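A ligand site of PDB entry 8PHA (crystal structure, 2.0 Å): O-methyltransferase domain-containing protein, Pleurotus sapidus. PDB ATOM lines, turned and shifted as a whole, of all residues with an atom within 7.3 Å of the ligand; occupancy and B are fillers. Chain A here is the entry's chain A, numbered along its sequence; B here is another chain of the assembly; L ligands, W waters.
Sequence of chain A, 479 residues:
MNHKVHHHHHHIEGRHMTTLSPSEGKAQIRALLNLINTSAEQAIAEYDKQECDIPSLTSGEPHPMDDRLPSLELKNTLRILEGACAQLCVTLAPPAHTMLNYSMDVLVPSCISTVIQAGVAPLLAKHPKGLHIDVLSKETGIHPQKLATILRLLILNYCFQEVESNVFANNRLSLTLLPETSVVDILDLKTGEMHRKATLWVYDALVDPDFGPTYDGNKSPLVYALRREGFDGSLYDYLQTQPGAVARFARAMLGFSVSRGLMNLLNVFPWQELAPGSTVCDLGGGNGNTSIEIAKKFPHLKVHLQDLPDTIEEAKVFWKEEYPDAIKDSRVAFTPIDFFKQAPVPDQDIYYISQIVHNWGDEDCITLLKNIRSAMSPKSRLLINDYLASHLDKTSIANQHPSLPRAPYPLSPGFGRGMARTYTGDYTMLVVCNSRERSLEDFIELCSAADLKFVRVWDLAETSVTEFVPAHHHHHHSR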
ATOM      1  N   LEU A 388      -0.476 -14.750 -29.107  1.00  0.00           N
ATOM      2  CA  LEU A 388      -1.137 -13.894 -28.114  1.00  0.00           C
ATOM      3  C   LEU A 388      -2.595 -13.764 -28.535  1.00  0.00           C
ATOM      4  O   LEU A 388      -2.945 -12.910 -29.346  1.00  0.00           O
ATOM      5  CB  LEU A 388      -0.435 -12.541 -28.012  1.00  0.00           C
ATOM      6  CG  LEU A 388       1.000 -12.603 -27.494  1.00  0.00           C
ATOM      7  CD1 LEU A 388       1.611 -11.196 -27.490  1.00  0.00           C
ATOM      8  CD2 LEU A 388       1.055 -13.209 -26.085  1.00  0.00           C
ATOM      9  N   ALA A 389      -3.442 -14.627 -27.977  1.00  0.00           N
ATOM     10  CA  ALA A 389      -4.873 -14.616 -28.287  1.00  0.00           C
ATOM     11  C   ALA A 389      -5.528 -13.479 -27.496  1.00  0.00           C
ATOM     12  O   ALA A 389      -6.237 -13.694 -26.509  1.00  0.00           O
ATOM     13  CB  ALA A 389      -5.500 -15.968 -28.002  1.00  0.00           C
ATOM     14  N   SER A 390      -5.300 -12.259 -27.974  1.00  0.00           N
ATOM     15  CA  SER A 390      -5.749 -11.017 -27.349  1.00  0.00           C
ATOM     16  C   SER A 390      -7.258 -10.831 -27.469  1.00  0.00           C
ATOM     17  O   SER A 390      -7.902 -11.265 -28.424  1.00  0.00           O
ATOM     18  CB  SER A 390      -5.100  -9.809 -28.025  1.00  0.00           C
ATOM     19  OG  SER A 390      -3.722 -10.038 -28.249  1.00  0.00           O
ATOM     20  N   HIS A 391      -7.807 -10.072 -26.518  1.00  0.00           N
ATOM     21  CA  HIS A 391      -9.201  -9.713 -26.596  1.00  0.00           C
ATOM     22  C   HIS A 391      -9.419  -8.727 -27.739  1.00  0.00           C
ATOM     23  O   HIS A 391      -8.513  -8.003 -28.150  1.00  0.00           O
ATOM     24  CB  HIS A 391      -9.681  -9.149 -25.258  1.00  0.00           C
ATOM     25  CG  HIS A 391      -9.551 -10.125 -24.139  1.00  0.00           C
ATOM     26  ND1 HIS A 391     -10.069  -9.902 -22.880  1.00  0.00           N
ATOM     27  CD2 HIS A 391      -8.936 -11.336 -24.084  1.00  0.00           C
ATOM     28  CE1 HIS A 391      -9.787 -10.933 -22.106  1.00  0.00           C
ATOM     29  NE2 HIS A 391      -9.110 -11.821 -22.808  1.00  0.00           N
ATOM     30  N   LEU A 392     -10.648  -8.723 -28.266  1.00  0.00           N
ATOM     31  CA  LEU A 392     -10.973  -8.044 -29.517  1.00  0.00           C
ATOM     32  C   LEU A 392     -11.851  -6.817 -29.296  1.00  0.00           C
ATOM     33  O   LEU A 392     -12.401  -6.280 -30.253  1.00  0.00           O
ATOM     34  CB  LEU A 392     -11.654  -9.017 -30.479  1.00  0.00           C
ATOM     35  CG  LEU A 392     -10.745 -10.200 -30.848  1.00  0.00           C
ATOM     36  CD1 LEU A 392     -11.419 -11.247 -31.748  1.00  0.00           C
ATOM     37  CD2 LEU A 392      -9.503  -9.657 -31.518  1.00  0.00           C
ATOM     38  N   ASP A 393     -11.967  -6.355 -28.053  1.00  0.00           N
ATOM     39  CA  ASP A 393     -12.749  -5.154 -27.817  1.00  0.00           C
ATOM     40  C   ASP A 393     -11.883  -3.921 -28.088  1.00  0.00           C
ATOM     41  O   ASP A 393     -10.660  -3.977 -28.058  1.00  0.00           O
ATOM     42  CB  ASP A 393     -13.264  -5.124 -26.388  1.00  0.00           C
ATOM     43  CG  ASP A 393     -12.144  -4.988 -25.371  1.00  0.00           C
ATOM     44  OD1 ASP A 393     -11.931  -3.846 -24.873  1.00  0.00           O
ATOM     45  OD2 ASP A 393     -11.452  -5.998 -25.104  1.00  0.00           O
ATOM     46  N   THR A 395     -11.369  -1.220 -26.353  1.00  0.00           N
ATOM     47  CA  THR A 395     -10.603  -0.670 -25.239  1.00  0.00           C
ATOM     48  C   THR A 395      -9.287  -1.430 -25.053  1.00  0.00           C
ATOM     49  O   THR A 395      -8.222  -0.808 -24.903  1.00  0.00           O
ATOM     50  CB  THR A 395     -11.444  -0.720 -23.966  1.00  0.00           C
ATOM     51  OG1 THR A 395     -12.746  -0.209 -24.255  1.00  0.00           O
ATOM     52  CG2 THR A 395     -10.799   0.118 -22.878  1.00  0.00           C
ATOM     53  N   SER A 396      -9.351  -2.759 -25.069  1.00  0.00           N
ATOM     54  CA  SER A 396      -8.134  -3.554 -24.947  1.00  0.00           C
ATOM     55  C   SER A 396      -7.167  -3.241 -26.088  1.00  0.00           C
ATOM     56  O   SER A 396      -5.955  -3.143 -25.883  1.00  0.00           O
ATOM     57  CB  SER A 396      -8.480  -5.041 -24.959  1.00  0.00           C
ATOM     58  OG  SER A 396      -9.319  -5.388 -23.866  1.00  0.00           O
ATOM     59  N   ILE A 397      -7.691  -3.064 -27.310  1.00  0.00           N
ATOM     60  CA  ILE A 397      -6.812  -2.819 -28.433  1.00  0.00           C
ATOM     61  C   ILE A 397      -6.228  -1.411 -28.371  1.00  0.00           C
ATOM     62  O   ILE A 397      -5.043  -1.208 -28.644  1.00  0.00           O
ATOM     63  CB  ILE A 397      -7.542  -3.085 -29.769  1.00  0.00           C
ATOM     64  CG1 ILE A 397      -7.826  -4.574 -29.912  1.00  0.00           C
ATOM     65  CG2 ILE A 397      -6.687  -2.594 -30.958  1.00  0.00           C
ATOM     66  CD1 ILE A 397      -9.010  -4.909 -30.825  1.00  0.00           C
ATOM     67  N   ALA A 398      -7.047  -0.420 -27.993  1.00  0.00           N
ATOM     68  CA  ALA A 398      -6.556   0.953 -27.927  1.00  0.00           C
ATOM     69  C   ALA A 398      -5.451   1.098 -26.897  1.00  0.00           C
ATOM     70  O   ALA A 398      -4.546   1.924 -27.081  1.00  0.00           O
ATOM     71  CB  ALA A 398      -7.706   1.908 -27.614  1.00  0.00           C
ATOM     72  N   ASN A 399      -5.498   0.322 -25.812  1.00  0.00           N
ATOM     73  CA  ASN A 399      -4.555   0.507 -24.709  1.00  0.00           C
ATOM     74  C   ASN A 399      -3.534  -0.625 -24.617  1.00  0.00           C
ATOM     75  O   ASN A 399      -2.903  -0.788 -23.578  1.00  0.00           O
ATOM     76  CB  ASN A 399      -5.328   0.656 -23.392  1.00  0.00           C
ATOM     77  CG  ASN A 399      -6.224   1.900 -23.378  1.00  0.00           C
ATOM     78  OD1 ASN A 399      -5.786   2.981 -23.054  1.00  0.00           O
ATOM     79  ND2 ASN A 399      -7.489   1.721 -23.743  1.00  0.00           N
ATOM     80  N   GLN A 400      -3.359  -1.396 -25.685  1.00  0.00           N
ATOM     81  CA  GLN A 400      -2.393  -2.477 -25.679  1.00  0.00           C
ATOM     82  C   GLN A 400      -0.974  -1.912 -25.542  1.00  0.00           C
ATOM     83  O   GLN A 400      -0.710  -0.735 -25.820  1.00  0.00           O
ATOM     84  CB  GLN A 400      -2.512  -3.310 -26.946  1.00  0.00           C
ATOM     85  CG  GLN A 400      -2.118  -2.537 -28.199  1.00  0.00           C
ATOM     86  CD  GLN A 400      -2.361  -3.294 -29.484  1.00  0.00           C
ATOM     87  OE1 GLN A 400      -3.097  -4.280 -29.524  1.00  0.00           O
ATOM     88  NE2 GLN A 400      -1.740  -2.822 -30.564  1.00  0.00           N
ATOM     89  N   HIS A 401      -0.066  -2.783 -25.138  1.00  0.00           N
ATOM     90  CA  HIS A 401       1.316  -2.372 -24.967  1.00  0.00           C
ATOM     91  C   HIS A 401       1.869  -1.795 -26.271  1.00  0.00           C
ATOM     92  O   HIS A 401       1.571  -2.309 -27.352  1.00  0.00           O
ATOM     93  CB  HIS A 401       2.181  -3.565 -24.533  1.00  0.00           C
ATOM     94  CG  HIS A 401       3.514  -3.149 -24.001  1.00  0.00           C
ATOM     95  ND1 HIS A 401       4.643  -3.080 -24.784  1.00  0.00           N
ATOM     96  CD2 HIS A 401       3.885  -2.764 -22.757  1.00  0.00           C
ATOM     97  CE1 HIS A 401       5.661  -2.679 -24.049  1.00  0.00           C
ATOM     98  NE2 HIS A 401       5.227  -2.474 -22.816  1.00  0.00           N
ATOM     99  N   LEU A 404       3.323  -3.944 -29.257  1.00  0.00           N
ATOM    100  CA  LEU A 404       2.451  -4.735 -30.111  1.00  0.00           C
ATOM    101  C   LEU A 404       2.203  -4.024 -31.433  1.00  0.00           C
ATOM    102  O   LEU A 404       2.092  -2.800 -31.473  1.00  0.00           O
ATOM    103  CB  LEU A 404       1.113  -4.992 -29.422  1.00  0.00           C
ATOM    104  CG  LEU A 404       1.147  -6.046 -28.319  1.00  0.00           C
ATOM    105  CD1 LEU A 404      -0.126  -6.026 -27.487  1.00  0.00           C
ATOM    106  CD2 LEU A 404       1.380  -7.416 -28.953  1.00  0.00           C
ATOM    107  N   TYR A 423      -6.318 -17.082 -33.869  1.00  0.00           N
ATOM    108  CA  TYR A 423      -7.617 -17.456 -33.350  1.00  0.00           C
ATOM    109  C   TYR A 423      -8.103 -18.788 -33.909  1.00  0.00           C
ATOM    110  O   TYR A 423      -8.821 -19.501 -33.201  1.00  0.00           O
ATOM    111  CB  TYR A 423      -8.613 -16.325 -33.648  1.00  0.00           C
ATOM    112  CG  TYR A 423      -8.153 -15.071 -32.904  1.00  0.00           C
ATOM    113  CD1 TYR A 423      -8.496 -14.869 -31.572  1.00  0.00           C
ATOM    114  CD2 TYR A 423      -7.279 -14.144 -33.500  1.00  0.00           C
ATOM    115  CE1 TYR A 423      -8.044 -13.762 -30.864  1.00  0.00           C
ATOM    116  CE2 TYR A 423      -6.825 -13.030 -32.803  1.00  0.00           C
ATOM    117  CZ  TYR A 423      -7.215 -12.845 -31.482  1.00  0.00           C
ATOM    118  OH  TYR A 423      -6.769 -11.766 -30.776  1.00  0.00           O
ATOM    119  N   ARG A 438      -3.172 -18.118 -25.013  1.00  0.00           N
ATOM    120  CA  ARG A 438      -3.422 -17.143 -23.962  1.00  0.00           C
ATOM    121  C   ARG A 438      -3.243 -15.731 -24.480  1.00  0.00           C
ATOM    122  O   ARG A 438      -2.494 -15.499 -25.440  1.00  0.00           O
ATOM    123  CB  ARG A 438      -2.502 -17.379 -22.757  1.00  0.00           C
ATOM    124  CG  ARG A 438      -2.988 -18.500 -21.822  1.00  0.00           C
ATOM    125  CD  ARG A 438      -1.904 -18.874 -20.819  1.00  0.00           C
ATOM    126  NE  ARG A 438      -2.298 -19.935 -19.906  1.00  0.00           N
ATOM    127  CZ  ARG A 438      -2.004 -21.218 -20.097  1.00  0.00           C
ATOM    128  NH1 ARG A 438      -1.374 -21.632 -21.187  1.00  0.00           N
ATOM    129  NH2 ARG A 438      -2.306 -22.100 -19.151  1.00  0.00           N
ATOM    130  N   SER A 439      -3.939 -14.794 -23.852  1.00  0.00           N
ATOM    131  CA  SER A 439      -3.761 -13.383 -24.143  1.00  0.00           C
ATOM    132  C   SER A 439      -2.485 -12.892 -23.490  1.00  0.00           C
ATOM    133  O   SER A 439      -1.908 -13.551 -22.622  1.00  0.00           O
ATOM    134  CB  SER A 439      -4.935 -12.566 -23.627  1.00  0.00           C
ATOM    135  OG  SER A 439      -4.926 -12.562 -22.207  1.00  0.00           O
ATOM    136  N   LEU A 440      -2.041 -11.695 -23.900  1.00  0.00           N
ATOM    137  CA  LEU A 440      -0.877 -11.100 -23.277  1.00  0.00           C
ATOM    138  C   LEU A 440      -1.075 -10.928 -21.780  1.00  0.00           C
ATOM    139  O   LEU A 440      -0.169 -11.208 -20.989  1.00  0.00           O
ATOM    140  CB  LEU A 440      -0.545  -9.756 -23.932  1.00  0.00           C
ATOM    141  CG  LEU A 440       0.695  -9.039 -23.404  1.00  0.00           C
ATOM    142  CD1 LEU A 440       1.899  -9.978 -23.350  1.00  0.00           C
ATOM    143  CD2 LEU A 440       1.028  -7.842 -24.274  1.00  0.00           C
ATOM    144  N   GLU A 441      -2.281 -10.525 -21.366  1.00  0.00           N
ATOM    145  CA  GLU A 441      -2.563 -10.347 -19.946  1.00  0.00           C
ATOM    146  C   GLU A 441      -2.471 -11.687 -19.199  1.00  0.00           C
ATOM    147  O   GLU A 441      -1.936 -11.739 -18.087  1.00  0.00           O
ATOM    148  CB  GLU A 441      -3.940  -9.694 -19.782  1.00  0.00           C
ATOM    149  CG  GLU A 441      -4.794 -10.205 -18.624  1.00  0.00           C
ATOM    150  CD  GLU A 441      -6.174  -9.507 -18.534  1.00  0.00           C
ATOM    151  OE1 GLU A 441      -6.267  -8.382 -17.988  1.00  0.00           O
ATOM    152  OE2 GLU A 441      -7.153 -10.085 -19.056  1.00  0.00           O
ATOM    153  N   ASP A 442      -2.958 -12.773 -19.803  1.00  0.00           N
ATOM    154  CA  ASP A 442      -2.839 -14.094 -19.170  1.00  0.00           C
ATOM    155  C   ASP A 442      -1.364 -14.451 -18.947  1.00  0.00           C
ATOM    156  O   ASP A 442      -0.994 -14.955 -17.880  1.00  0.00           O
ATOM    157  CB  ASP A 442      -3.509 -15.175 -20.032  1.00  0.00           C
ATOM    158  CG  ASP A 442      -5.001 -14.964 -20.220  1.00  0.00           C
ATOM    159  OD1 ASP A 442      -5.660 -14.362 -19.333  1.00  0.00           O
ATOM    160  OD2 ASP A 442      -5.509 -15.392 -21.280  1.00  0.00           O
ATOM    161  N   PHE A 443      -0.529 -14.227 -19.970  1.00  0.00           N
ATOM    162  CA  PHE A 443       0.905 -14.475 -19.852  1.00  0.00           C
ATOM    163  C   PHE A 443       1.534 -13.633 -18.763  1.00  0.00           C
ATOM    164  O   PHE A 443       2.363 -14.106 -17.971  1.00  0.00           O
ATOM    165  CB  PHE A 443       1.595 -14.185 -21.180  1.00  0.00           C
ATOM    166  CG  PHE A 443       1.560 -15.309 -22.160  1.00  0.00           C
ATOM    167  CD1 PHE A 443       2.433 -16.371 -22.032  1.00  0.00           C
ATOM    168  CD2 PHE A 443       0.675 -15.286 -23.222  1.00  0.00           C
ATOM    169  CE1 PHE A 443       2.409 -17.410 -22.934  1.00  0.00           C
ATOM    170  CE2 PHE A 443       0.652 -16.317 -24.135  1.00  0.00           C
ATOM    171  CZ  PHE A 443       1.529 -17.389 -23.988  1.00  0.00           C
ATOM    172  N   ILE A 444       1.203 -12.339 -18.743  1.00  0.00           N
ATOM    173  CA  ILE A 444       1.793 -11.447 -17.764  1.00  0.00           C
ATOM    174  C   ILE A 444       1.420 -11.881 -16.359  1.00  0.00           C
ATOM    175  O   ILE A 444       2.249 -11.833 -15.438  1.00  0.00           O
ATOM    176  CB  ILE A 444       1.370  -9.991 -18.036  1.00  0.00           C
ATOM    177  CG1 ILE A 444       2.022  -9.497 -19.332  1.00  0.00           C
ATOM    178  CG2 ILE A 444       1.744  -9.103 -16.857  1.00  0.00           C
ATOM    179  CD1 ILE A 444       1.545  -8.147 -19.807  1.00  0.00           C
ATOM    180  N   ARG B 152     -14.460 -15.459 -30.178  1.00  0.00           N
ATOM    181  CA  ARG B 152     -13.437 -14.580 -30.742  1.00  0.00           C
ATOM    182  C   ARG B 152     -13.054 -15.005 -32.137  1.00  0.00           C
ATOM    183  O   ARG B 152     -12.758 -14.133 -32.969  1.00  0.00           O
ATOM    184  CB  ARG B 152     -12.206 -14.512 -29.834  1.00  0.00           C
ATOM    185  CG  ARG B 152     -12.484 -13.700 -28.545  1.00  0.00           C
ATOM    186  CD  ARG B 152     -11.244 -13.216 -27.806  1.00  0.00           C
ATOM    187  NE  ARG B 152     -11.652 -12.463 -26.629  1.00  0.00           N
ATOM    188  CZ  ARG B 152     -11.718 -12.963 -25.407  1.00  0.00           C
ATOM    189  NH1 ARG B 152     -11.319 -14.200 -25.134  1.00  0.00           N
ATOM    190  NH2 ARG B 152     -12.214 -12.213 -24.420  1.00  0.00           N
ATOM    191  N   GLU B 162     -16.984  -7.975 -29.486  1.00  0.00           N
ATOM    192  CA  GLU B 162     -16.563  -7.836 -28.093  1.00  0.00           C
ATOM    193  C   GLU B 162     -16.629  -6.339 -27.753  1.00  0.00           C
ATOM    194  O   GLU B 162     -15.854  -5.554 -28.306  1.00  0.00           O
ATOM    195  CB  GLU B 162     -15.167  -8.422 -27.877  1.00  0.00           C
ATOM    196  CG  GLU B 162     -14.838  -8.715 -26.399  1.00  0.00           C
ATOM    197  CD  GLU B 162     -13.576  -9.551 -26.196  1.00  0.00           C
ATOM    198  OE1 GLU B 162     -13.009 -10.062 -27.180  1.00  0.00           O
ATOM    199  OE2 GLU B 162     -13.157  -9.718 -25.034  1.00  0.00           O
ATOM    200  N   SER B 165     -13.740  -6.023 -22.613  1.00  0.00           N
ATOM    201  CA  SER B 165     -13.043  -7.279 -22.378  1.00  0.00           C
ATOM    202  C   SER B 165     -13.984  -8.314 -21.764  1.00  0.00           C
ATOM    203  O   SER B 165     -14.544  -8.099 -20.690  1.00  0.00           O
ATOM    204  CB  SER B 165     -11.836  -7.044 -21.470  1.00  0.00           C
ATOM    205  OG  SER B 165     -11.135  -8.257 -21.239  1.00  0.00           O
HETATM  206  N1  LIG L   1      -5.712  -6.509 -24.416  1.00  0.00           N
HETATM  207  C1  LIG L   1      -5.740  -7.198 -23.146  1.00  0.00           C
HETATM  208  C2  LIG L   1      -7.118  -7.233 -22.455  1.00  0.00           C
HETATM  209  C3  LIG L   1      -6.888  -6.811 -21.015  1.00  0.00           C
HETATM  210  C4  LIG L   1      -8.020  -5.889 -20.549  1.00  0.00           C
HETATM  211  N2  LIG L   1      -7.535  -5.127 -19.407  1.00  0.00           N
HETATM  212  C5  LIG L   1      -5.296  -8.560 -23.501  1.00  0.00           C
HETATM  213  O1  LIG L   1      -4.272  -9.041 -22.972  1.00  0.00           O
HETATM  214  O2  LIG L   1      -5.975  -9.173 -24.342  1.00  0.00           O
HETATM  215  O   HOH W   1      -6.233  -6.818 -27.097  1.00  0.00           O
HETATM  216  O   HOH W   2      -4.842  -4.225 -23.493  1.00  0.00           O
HETATM  217  O   HOH W   3      -2.911  -6.765 -25.342  1.00  0.00           O
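Merely in contact with the ligand: Ser 390, Ser 396, Ser 439, Leu 440 and Ser 165 of chain B. Within 4 Å of the ligand: Ser 390, His 391, Ser 396, Ser 439, Leu 440, Glu 441 and Ser 165 of chain B. The nearest printed residue that does not touch the ligand is Ile 397 (4.9 Å).
The side-chain hydroxyl of Ser 439 is in hydrogen-bond range of the side-chain carboxylate of Asp 442, 3.0 Å away. The side-chain hydroxyl (OG) of Ser 396 lies within hydrogen-bond range of the side-chain carboxylate (OD2) of Asp 393. The side-chain hydroxyl (OH) of Tyr 423 is in hydrogen-bond range of the backbone carbonyl oxygen (O) of Ser 390. The backbone NH (N) of Ser 165 of chain B lies close to the side-chain carboxylate (OD2) of Asp 393. The backbone NH of Glu 441 lies close to the side-chain hydroxyl of Ser 439 (3.4 Å). OG of Ser 165 of chain B lies within hydrogen-bond range of ND1 of His 391, 2.6 Å away. The backbone carbonyl oxygen of Leu 388 lies within hydrogen-bond range of the side-chain hydroxyl of Ser 390, 3.2 Å away.
Water W2 lies within hydrogen-bond range of N1 of the ligand (2.6 Å) and O of Ser 396 (2.8 Å). Water W1 bridges N1 of the ligand (2.7 Å) and O of His 391 (2.8 Å).
N of His 391 sits at hydrogen-bond distance from O2 of the ligand. N2 of the ligand lies within salt-bridge range of OE1 of Glu 441 (3.8 Å). N of Glu 441 sits at hydrogen-bond distance from O1 of the ligand.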
